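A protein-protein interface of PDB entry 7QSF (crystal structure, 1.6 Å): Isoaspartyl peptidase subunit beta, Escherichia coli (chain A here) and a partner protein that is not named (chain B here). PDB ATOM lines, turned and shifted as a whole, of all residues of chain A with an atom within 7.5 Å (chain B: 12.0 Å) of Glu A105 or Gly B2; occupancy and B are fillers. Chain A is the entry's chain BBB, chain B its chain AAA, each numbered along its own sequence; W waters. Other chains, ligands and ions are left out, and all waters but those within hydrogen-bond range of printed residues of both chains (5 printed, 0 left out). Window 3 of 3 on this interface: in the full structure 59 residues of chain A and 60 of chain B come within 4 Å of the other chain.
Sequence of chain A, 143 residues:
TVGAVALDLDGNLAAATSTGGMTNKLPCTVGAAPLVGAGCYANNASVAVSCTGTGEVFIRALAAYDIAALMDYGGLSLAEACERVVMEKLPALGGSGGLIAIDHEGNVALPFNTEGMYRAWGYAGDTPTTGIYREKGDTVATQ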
ATOM      1  N   LEU A   7      30.944   0.221  21.073  1.00  0.00           N
ATOM      2  CA  LEU A   7      30.387  -0.836  20.181  1.00  0.00           C
ATOM      3  C   LEU A   7      31.109  -0.716  18.841  1.00  0.00           C
ATOM      4  O   LEU A   7      31.119   0.398  18.299  1.00  0.00           O
ATOM      5  CB  LEU A   7      28.870  -0.714  19.974  1.00  0.00           C
ATOM      6  CG  LEU A   7      28.249  -1.684  18.956  1.00  0.00           C
ATOM      7  CD1 LEU A   7      28.307  -3.123  19.465  1.00  0.00           C
ATOM      8  CD2 LEU A   7      26.808  -1.305  18.671  1.00  0.00           C
ATOM      9  N   ASP A   8      31.697  -1.801  18.338  1.00  0.00           N
ATOM     10  CA  ASP A   8      32.568  -1.774  17.129  1.00  0.00           C
ATOM     11  C   ASP A   8      31.756  -2.286  15.922  1.00  0.00           C
ATOM     12  O   ASP A   8      30.595  -2.667  16.067  1.00  0.00           O
ATOM     13  CB  ASP A   8      33.935  -2.443  17.380  1.00  0.00           C
ATOM     14  CG  ASP A   8      33.926  -3.955  17.556  1.00  0.00           C
ATOM     15  OD1 ASP A   8      32.964  -4.598  17.098  1.00  0.00           O
ATOM     16  OD2 ASP A   8      34.888  -4.505  18.137  1.00  0.00           O
ATOM     17  N   LEU A   9      32.363  -2.260  14.734  1.00  0.00           N
ATOM     18  CA  LEU A   9      31.655  -2.677  13.496  1.00  0.00           C
ATOM     19  C   LEU A   9      31.378  -4.185  13.463  1.00  0.00           C
ATOM     20  O   LEU A   9      30.525  -4.636  12.627  1.00  0.00           O
ATOM     21  CB  LEU A   9      32.510  -2.236  12.316  1.00  0.00           C
ATOM     22  CG  LEU A   9      32.417  -0.750  11.994  1.00  0.00           C
ATOM     23  CD1 LEU A   9      33.408  -0.427  10.887  1.00  0.00           C
ATOM     24  CD2 LEU A   9      30.978  -0.368  11.617  1.00  0.00           C
ATOM     25  N   ASP A  10      32.082  -4.957  14.289  1.00  0.00           N
ATOM     26  CA  ASP A  10      31.834  -6.420  14.421  1.00  0.00           C
ATOM     27  C   ASP A  10      30.772  -6.725  15.491  1.00  0.00           C
ATOM     28  O   ASP A  10      30.532  -7.910  15.735  1.00  0.00           O
ATOM     29  CB  ASP A  10      33.163  -7.122  14.700  1.00  0.00           C
ATOM     30  CG  ASP A  10      34.150  -6.913  13.563  1.00  0.00           C
ATOM     31  OD1 ASP A  10      33.775  -7.152  12.372  1.00  0.00           O
ATOM     32  OD2 ASP A  10      35.258  -6.447  13.864  1.00  0.00           O
ATOM     33  N   GLY A  11      30.160  -5.712  16.116  1.00  0.00           N
ATOM     34  CA  GLY A  11      29.083  -5.887  17.123  1.00  0.00           C
ATOM     35  C   GLY A  11      29.601  -6.198  18.517  1.00  0.00           C
ATOM     36  O   GLY A  11      28.808  -6.685  19.380  1.00  0.00           O
ATOM     37  N   LEU A  13      31.129  -5.331  22.285  1.00  0.00           N
ATOM     38  CA  LEU A  13      31.031  -4.289  23.352  1.00  0.00           C
ATOM     39  C   LEU A  13      32.255  -4.327  24.278  1.00  0.00           C
ATOM     40  O   LEU A  13      32.739  -5.467  24.574  1.00  0.00           O
ATOM     41  CB  LEU A  13      29.747  -4.525  24.141  1.00  0.00           C
ATOM     42  CG  LEU A  13      28.427  -4.139  23.447  1.00  0.00           C
ATOM     43  CD1 LEU A  13      27.219  -4.554  24.277  1.00  0.00           C
ATOM     44  CD2 LEU A  13      28.372  -2.646  23.169  1.00  0.00           C
ATOM     45  N   ASN A  44      28.428  -8.845  25.399  1.00  0.00           N
ATOM     46  CA  ASN A  44      27.876  -8.721  24.019  1.00  0.00           C
ATOM     47  C   ASN A  44      26.356  -8.993  23.969  1.00  0.00           C
ATOM     48  O   ASN A  44      25.722  -8.421  23.050  1.00  0.00           O
ATOM     49  CB  ASN A  44      28.620  -9.604  23.006  1.00  0.00           C
ATOM     50  CG  ASN A  44      29.894  -8.959  22.496  1.00  0.00           C
ATOM     51  OD1 ASN A  44      30.290  -7.899  22.981  1.00  0.00           O
ATOM     52  ND2 ASN A  44      30.564  -9.592  21.538  1.00  0.00           N
ATOM     53  N   SER A  46      24.112  -7.896  26.136  1.00  0.00           N
ATOM     54  CA  SER A  46      23.344  -6.793  26.761  1.00  0.00           C
ATOM     55  C   SER A  46      24.047  -5.452  26.554  1.00  0.00           C
ATOM     56  O   SER A  46      23.604  -4.680  25.677  1.00  0.00           O
ATOM     57  CB  SER A  46      23.125  -7.079  28.216  1.00  0.00           C
ATOM     58  OG  SER A  46      24.329  -7.513  28.820  1.00  0.00           O
ATOM     59  N   MET A  71      18.185  -5.439  31.757  1.00  0.00           N
ATOM     60  CA  MET A  71      17.945  -5.494  30.292  1.00  0.00           C
ATOM     61  C   MET A  71      17.789  -6.952  29.867  1.00  0.00           C
ATOM     62  O   MET A  71      16.761  -7.267  29.268  1.00  0.00           O
ATOM     63  CB  MET A  71      19.076  -4.828  29.510  1.00  0.00           C
ATOM     64  CG  MET A  71      19.112  -3.329  29.761  1.00  0.00           C
ATOM     65  SD  MET A  71      20.365  -2.522  28.733  1.00  0.00           S
ATOM     66  CE  MET A  71      19.648  -2.779  27.115  1.00  0.00           C
ATOM     67  N   ILE A 102      26.394   1.700  26.646  1.00  0.00           N
ATOM     68  CA  ILE A 102      26.035   1.380  25.233  1.00  0.00           C
ATOM     69  C   ILE A 102      25.517  -0.055  25.165  1.00  0.00           C
ATOM     70  O   ILE A 102      26.159  -0.957  25.710  1.00  0.00           O
ATOM     71  CB  ILE A 102      27.211   1.594  24.254  1.00  0.00           C
ATOM     72  CG1 ILE A 102      27.651   3.055  24.166  1.00  0.00           C
ATOM     73  CG2 ILE A 102      26.882   1.042  22.862  1.00  0.00           C
ATOM     74  CD1 ILE A 102      29.040   3.256  23.540  1.00  0.00           C
ATOM     75  N   ASP A 103      24.341  -0.245  24.547  1.00  0.00           N
ATOM     76  CA  ASP A 103      23.772  -1.609  24.401  1.00  0.00           C
ATOM     77  C   ASP A 103      24.183  -2.256  23.066  1.00  0.00           C
ATOM     78  O   ASP A 103      24.781  -1.611  22.203  1.00  0.00           O
ATOM     79  CB  ASP A 103      22.269  -1.615  24.662  1.00  0.00           C
ATOM     80  CG  ASP A 103      21.352  -1.105  23.559  1.00  0.00           C
ATOM     81  OD1 ASP A 103      21.828  -0.876  22.423  1.00  0.00           O
ATOM     82  OD2 ASP A 103      20.139  -0.990  23.852  1.00  0.00           O
ATOM     83  N   HIS A 104      23.878  -3.537  22.926  1.00  0.00           N
ATOM     84  CA  HIS A 104      24.263  -4.365  21.759  1.00  0.00           C
ATOM     85  C   HIS A 104      23.625  -3.842  20.462  1.00  0.00           C
ATOM     86  O   HIS A 104      24.111  -4.233  19.397  1.00  0.00           O
ATOM     87  CB  HIS A 104      23.991  -5.831  22.071  1.00  0.00           C
ATOM     88  CG  HIS A 104      22.548  -6.190  22.177  1.00  0.00           C
ATOM     89  ND1 HIS A 104      21.837  -6.735  21.110  1.00  0.00           N
ATOM     90  CD2 HIS A 104      21.688  -6.133  23.214  1.00  0.00           C
ATOM     91  CE1 HIS A 104      20.594  -6.972  21.483  1.00  0.00           C
ATOM     92  NE2 HIS A 104      20.471  -6.615  22.771  1.00  0.00           N
ATOM     93  N   GLU A 105      22.627  -2.956  20.504  1.00  0.00           N
ATOM     94  CA  GLU A 105      21.978  -2.375  19.294  1.00  0.00           C
ATOM     95  C   GLU A 105      22.552  -0.978  19.002  1.00  0.00           C
ATOM     96  O   GLU A 105      22.136  -0.343  17.998  1.00  0.00           O
ATOM     97  CB  GLU A 105      20.460  -2.343  19.496  1.00  0.00           C
ATOM     98  CG  GLU A 105      19.835  -3.718  19.716  1.00  0.00           C
ATOM     99  CD  GLU A 105      18.342  -3.699  20.021  1.00  0.00           C
ATOM    100  OE1 GLU A 105      17.541  -3.458  19.093  1.00  0.00           O
ATOM    101  OE2 GLU A 105      17.981  -3.888  21.196  1.00  0.00           O
ATOM    102  N   GLY A 106      23.463  -0.496  19.842  1.00  0.00           N
ATOM    103  CA  GLY A 106      24.109   0.825  19.674  1.00  0.00           C
ATOM    104  C   GLY A 106      23.288   1.994  20.204  1.00  0.00           C
ATOM    105  O   GLY A 106      23.634   3.158  19.852  1.00  0.00           O
ATOM    106  N   ASN A 107      22.303   1.737  21.064  1.00  0.00           N
ATOM    107  CA  ASN A 107      21.659   2.794  21.890  1.00  0.00           C
ATOM    108  C   ASN A 107      22.680   3.256  22.931  1.00  0.00           C
ATOM    109  O   ASN A 107      23.453   2.382  23.408  1.00  0.00           O
ATOM    110  CB  ASN A 107      20.379   2.332  22.591  1.00  0.00           C
ATOM    111  CG  ASN A 107      19.325   1.894  21.601  1.00  0.00           C
ATOM    112  OD1 ASN A 107      18.961   2.662  20.709  1.00  0.00           O
ATOM    113  ND2 ASN A 107      18.906   0.646  21.699  1.00  0.00           N
ATOM    114  N   VAL A 108      22.666   4.554  23.244  1.00  0.00           N
ATOM    115  CA  VAL A 108      23.642   5.191  24.180  1.00  0.00           C
ATOM    116  C   VAL A 108      22.853   5.936  25.259  1.00  0.00           C
ATOM    117  O   VAL A 108      21.749   6.513  24.948  1.00  0.00           O
ATOM    118  CB  VAL A 108      24.675   6.090  23.461  1.00  0.00           C
ATOM    119  CG1 VAL A 108      24.100   7.415  22.993  1.00  0.00           C
ATOM    120  CG2 VAL A 108      25.910   6.345  24.315  1.00  0.00           C
ATOM    121  N   TYR A 123      28.889   8.735  17.235  1.00  0.00           N
ATOM    122  CA  TYR A 123      28.886   7.637  16.246  1.00  0.00           C
ATOM    123  C   TYR A 123      30.133   7.753  15.367  1.00  0.00           C
ATOM    124  O   TYR A 123      30.599   8.884  15.070  1.00  0.00           O
ATOM    125  CB  TYR A 123      27.657   7.715  15.342  1.00  0.00           C
ATOM    126  CG  TYR A 123      26.327   7.680  16.050  1.00  0.00           C
ATOM    127  CD1 TYR A 123      25.925   6.585  16.793  1.00  0.00           C
ATOM    128  CD2 TYR A 123      25.435   8.730  15.917  1.00  0.00           C
ATOM    129  CE1 TYR A 123      24.669   6.543  17.400  1.00  0.00           C
ATOM    130  CE2 TYR A 123      24.197   8.716  16.537  1.00  0.00           C
ATOM    131  CZ  TYR A 123      23.805   7.613  17.272  1.00  0.00           C
ATOM    132  OH  TYR A 123      22.568   7.603  17.855  1.00  0.00           O
ATOM    133  N   GLY B   2      23.754  -2.098  14.685  1.00  0.00           N
ATOM    134  CA  GLY B   2      23.751  -0.681  15.071  1.00  0.00           C
ATOM    135  C   GLY B   2      25.047   0.013  14.683  1.00  0.00           C
ATOM    136  O   GLY B   2      26.039  -0.674  14.381  1.00  0.00           O
ATOM    137  N   LYS B   3      25.010   1.335  14.589  1.00  0.00           N
ATOM    138  CA  LYS B   3      26.196   2.133  14.212  1.00  0.00           C
ATOM    139  C   LYS B   3      27.265   1.914  15.291  1.00  0.00           C
ATOM    140  O   LYS B   3      26.874   1.794  16.488  1.00  0.00           O
ATOM    141  CB  LYS B   3      25.904   3.634  14.161  1.00  0.00           C
ATOM    142  CG  LYS B   3      24.679   4.095  13.382  1.00  0.00           C
ATOM    143  CD  LYS B   3      24.267   5.477  13.854  1.00  0.00           C
ATOM    144  CE  LYS B   3      23.229   6.165  13.008  1.00  0.00           C
ATOM    145  NZ  LYS B   3      23.634   7.565  12.731  1.00  0.00           N
ATOM    146  N   ALA B   4      28.539   1.867  14.900  1.00  0.00           N
ATOM    147  CA  ALA B   4      29.670   1.858  15.856  1.00  0.00           C
ATOM    148  C   ALA B   4      29.678   3.189  16.607  1.00  0.00           C
ATOM    149  O   ALA B   4      29.336   4.248  16.030  1.00  0.00           O
ATOM    150  CB  ALA B   4      31.006   1.581  15.204  1.00  0.00           C
ATOM    151  N   VAL B   5      30.029   3.140  17.894  1.00  0.00           N
ATOM    152  CA  VAL B   5      29.821   4.320  18.775  1.00  0.00           C
ATOM    153  C   VAL B   5      30.724   4.217  20.008  1.00  0.00           C
ATOM    154  O   VAL B   5      31.008   3.118  20.490  1.00  0.00           O
ATOM    155  CB  VAL B   5      28.334   4.508  19.146  1.00  0.00           C
ATOM    156  CG1 VAL B   5      27.691   3.305  19.822  1.00  0.00           C
ATOM    157  CG2 VAL B   5      28.134   5.776  19.969  1.00  0.00           C
ATOM    158  N   ILE B   6      31.108   5.382  20.526  1.00  0.00           N
ATOM    159  CA  ILE B   6      31.934   5.522  21.757  1.00  0.00           C
ATOM    160  C   ILE B   6      31.275   6.551  22.664  1.00  0.00           C
ATOM    161  O   ILE B   6      30.783   7.554  22.139  1.00  0.00           O
ATOM    162  CB  ILE B   6      33.370   5.942  21.410  1.00  0.00           C
ATOM    163  CG1 ILE B   6      34.211   6.091  22.675  1.00  0.00           C
ATOM    164  CG2 ILE B   6      33.390   7.196  20.544  1.00  0.00           C
ATOM    165  CD1 ILE B   6      35.674   6.351  22.481  1.00  0.00           C
ATOM    166  N   LEU B  43      37.194   3.457  15.531  1.00  0.00           N
ATOM    167  CA  LEU B  43      35.972   2.650  15.193  1.00  0.00           C
ATOM    168  C   LEU B  43      35.720   2.664  13.672  1.00  0.00           C
ATOM    169  O   LEU B  43      35.440   1.584  13.098  1.00  0.00           O
ATOM    170  CB  LEU B  43      34.759   3.140  16.010  1.00  0.00           C
ATOM    171  CG  LEU B  43      34.833   2.869  17.528  1.00  0.00           C
ATOM    172  CD1 LEU B  43      33.780   3.654  18.303  1.00  0.00           C
ATOM    173  CD2 LEU B  43      34.785   1.381  17.879  1.00  0.00           C
ATOM    174  N   GLU B  44      35.857   3.823  13.039  1.00  0.00           N
ATOM    175  CA  GLU B  44      35.520   3.994  11.607  1.00  0.00           C
ATOM    176  C   GLU B  44      36.534   3.195  10.790  1.00  0.00           C
ATOM    177  O   GLU B  44      36.171   2.658   9.710  1.00  0.00           O
ATOM    178  CB  GLU B  44      35.515   5.475  11.260  1.00  0.00           C
ATOM    179  CG  GLU B  44      34.934   5.730   9.877  1.00  0.00           C
ATOM    180  CD  GLU B  44      35.029   7.166   9.401  1.00  0.00           C
ATOM    181  OE1 GLU B  44      34.750   7.380   8.215  1.00  0.00           O
ATOM    182  OE2 GLU B  44      35.387   8.052  10.204  1.00  0.00           O
ATOM    183  N   GLY B  46      37.740   0.373  11.622  1.00  0.00           N
ATOM    184  CA  GLY B  46      37.479  -1.058  11.906  1.00  0.00           C
ATOM    185  C   GLY B  46      38.210  -1.620  13.129  1.00  0.00           C
ATOM    186  O   GLY B  46      38.181  -2.879  13.307  1.00  0.00           O
ATOM    187  N   GLU B  47      38.813  -0.780  13.988  1.00  0.00           N
ATOM    188  CA  GLU B  47      39.516  -1.240  15.220  1.00  0.00           C
ATOM    189  C   GLU B  47      38.511  -1.764  16.269  1.00  0.00           C
ATOM    190  O   GLU B  47      37.339  -1.402  16.231  1.00  0.00           O
ATOM    191  CB  GLU B  47      40.375  -0.111  15.808  1.00  0.00           C
ATOM    192  CG  GLU B  47      41.536   0.302  14.891  1.00  0.00           C
ATOM    193  CD  GLU B  47      42.450  -0.830  14.463  1.00  0.00           C
ATOM    194  OE1 GLU B  47      42.614  -1.032  13.233  1.00  0.00           O
ATOM    195  OE2 GLU B  47      43.046  -1.520  15.338  1.00  0.00           O
ATOM    196  N   ALA B  49      36.372  -2.640  19.817  1.00  0.00           N
ATOM    197  CA  ALA B  49      35.816  -1.888  20.974  1.00  0.00           C
ATOM    198  C   ALA B  49      36.811  -1.993  22.143  1.00  0.00           C
ATOM    199  O   ALA B  49      37.062  -0.994  22.807  1.00  0.00           O
ATOM    200  CB  ALA B  49      34.435  -2.403  21.335  1.00  0.00           C
HETATM  201  O   HOH W   1      24.786   3.494  17.540  1.00  0.00           O
HETATM  202  O   HOH W   2      34.991  -0.839  14.501  1.00  0.00           O
HETATM  203  O   HOH W   3      36.535  -5.661  20.931  1.00  0.00           O
HETATM  204  O   HOH W   4      27.915  -2.651  15.144  1.00  0.00           O
HETATM  205  O   HOH W   5      35.742  -4.408  11.836  1.00  0.00           O
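The backbone NH (N) of Leu A7 sits at hydrogen-bond distance from the backbone carbonyl oxygen (O) of Val B5, 3.0 Å away.
The side-chain carboxylate of Asp A8 sits at hydrogen-bond distance from the backbone NH of Ala B49, at 2.9 Å.
N of Asp A10 lies within hydrogen-bond range of OD1 of Asp A8 (3.0 Å).
The side-chain carboxylate (OD1) of Asp A103 lies within hydrogen-bond range of the backbone NH (N) of Glu A105, at 2.9 Å.
N of Gly A11 lies within hydrogen-bond range of OD1 of Asp A8 (3.2 Å).
Among the printed residues, merely in contact across the chains: Leu A7 with Ala B4, Glu A105 with Gly B2, Tyr A123 with Ala B4, Tyr A123 with Lys B3, Leu A9 with Leu B43, Ile A102 with Val B5, Asp A8 with Glu B47, Leu A7 with Lys B3, Leu A7 with Leu B43, Asp A8 with Leu B43 and Tyr A123 with Val B5.
Of the printed residues of chain B, Asp A8 touches Leu B43 (3.9 Å), Glu B47 (3.7 Å) and Ala B49 (2.9 Å).
Printed residues of chain B within 4 Å of Leu A9: Leu B43.
No residue of chain B comes within 4 Å of Gly A11.
Printed residues of chain B within 4 Å of Ile A102: Val B5.
No residue of chain B comes within 4 Å of Asp A103.
Printed residues of chain B within 4 Å of Glu A105: Gly B2.
No residue of chain B comes within 4 Å of Gly A106.
No residue of chain B comes within 4 Å of Asn A107.
Of the printed residues of chain A, Gly B2 touches Glu A105.
Of the printed residues of chain A, Lys B3 touches Leu A7 and Tyr A123.
The nearest printed residue of chain A that does not touch Gly B2 is Leu A7 (4.4 Å).
Of the 17 printed residues of chain A, 6 touch a printed residue of chain B.
Hydrophobic or aromatic side chains of chain A within 4 Å of the printed part of chain B: Leu A7, Leu A9, Ile A102 and Tyr A123.
Along chain A the printed residues that touch a printed residue of chain B span positions 7 to 123.
Of the 10 printed residues of chain B, 7 touch a printed residue of chain A.
Hydrophobic or aromatic side chains of chain B within 4 Å of the printed part of chain A: Ala B4, Val B5, Leu B43 and Ala B49.
Water W1 lies within hydrogen-bond range of O of Gly A106 (2.6 Å) and O of Lys B3 (2.9 Å).
Water W4 bridges O of Gly B2 (2.8 Å) and O of Asp A8 (2.8 Å).
Water W2 lies within hydrogen-bond range of O of Leu B43 (2.8 Å), O of Glu B47 (3.0 Å) and N of Leu A9 (3.0 Å).
Water W5 lies within hydrogen-bond range of the side-chain carboxylate of Asp A10 and the backbone carbonyl oxygen of Gly B46.
Water W3 bridges N of Ala B49 (3.2 Å) and OD2 of Asp A8 (3.4 Å).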
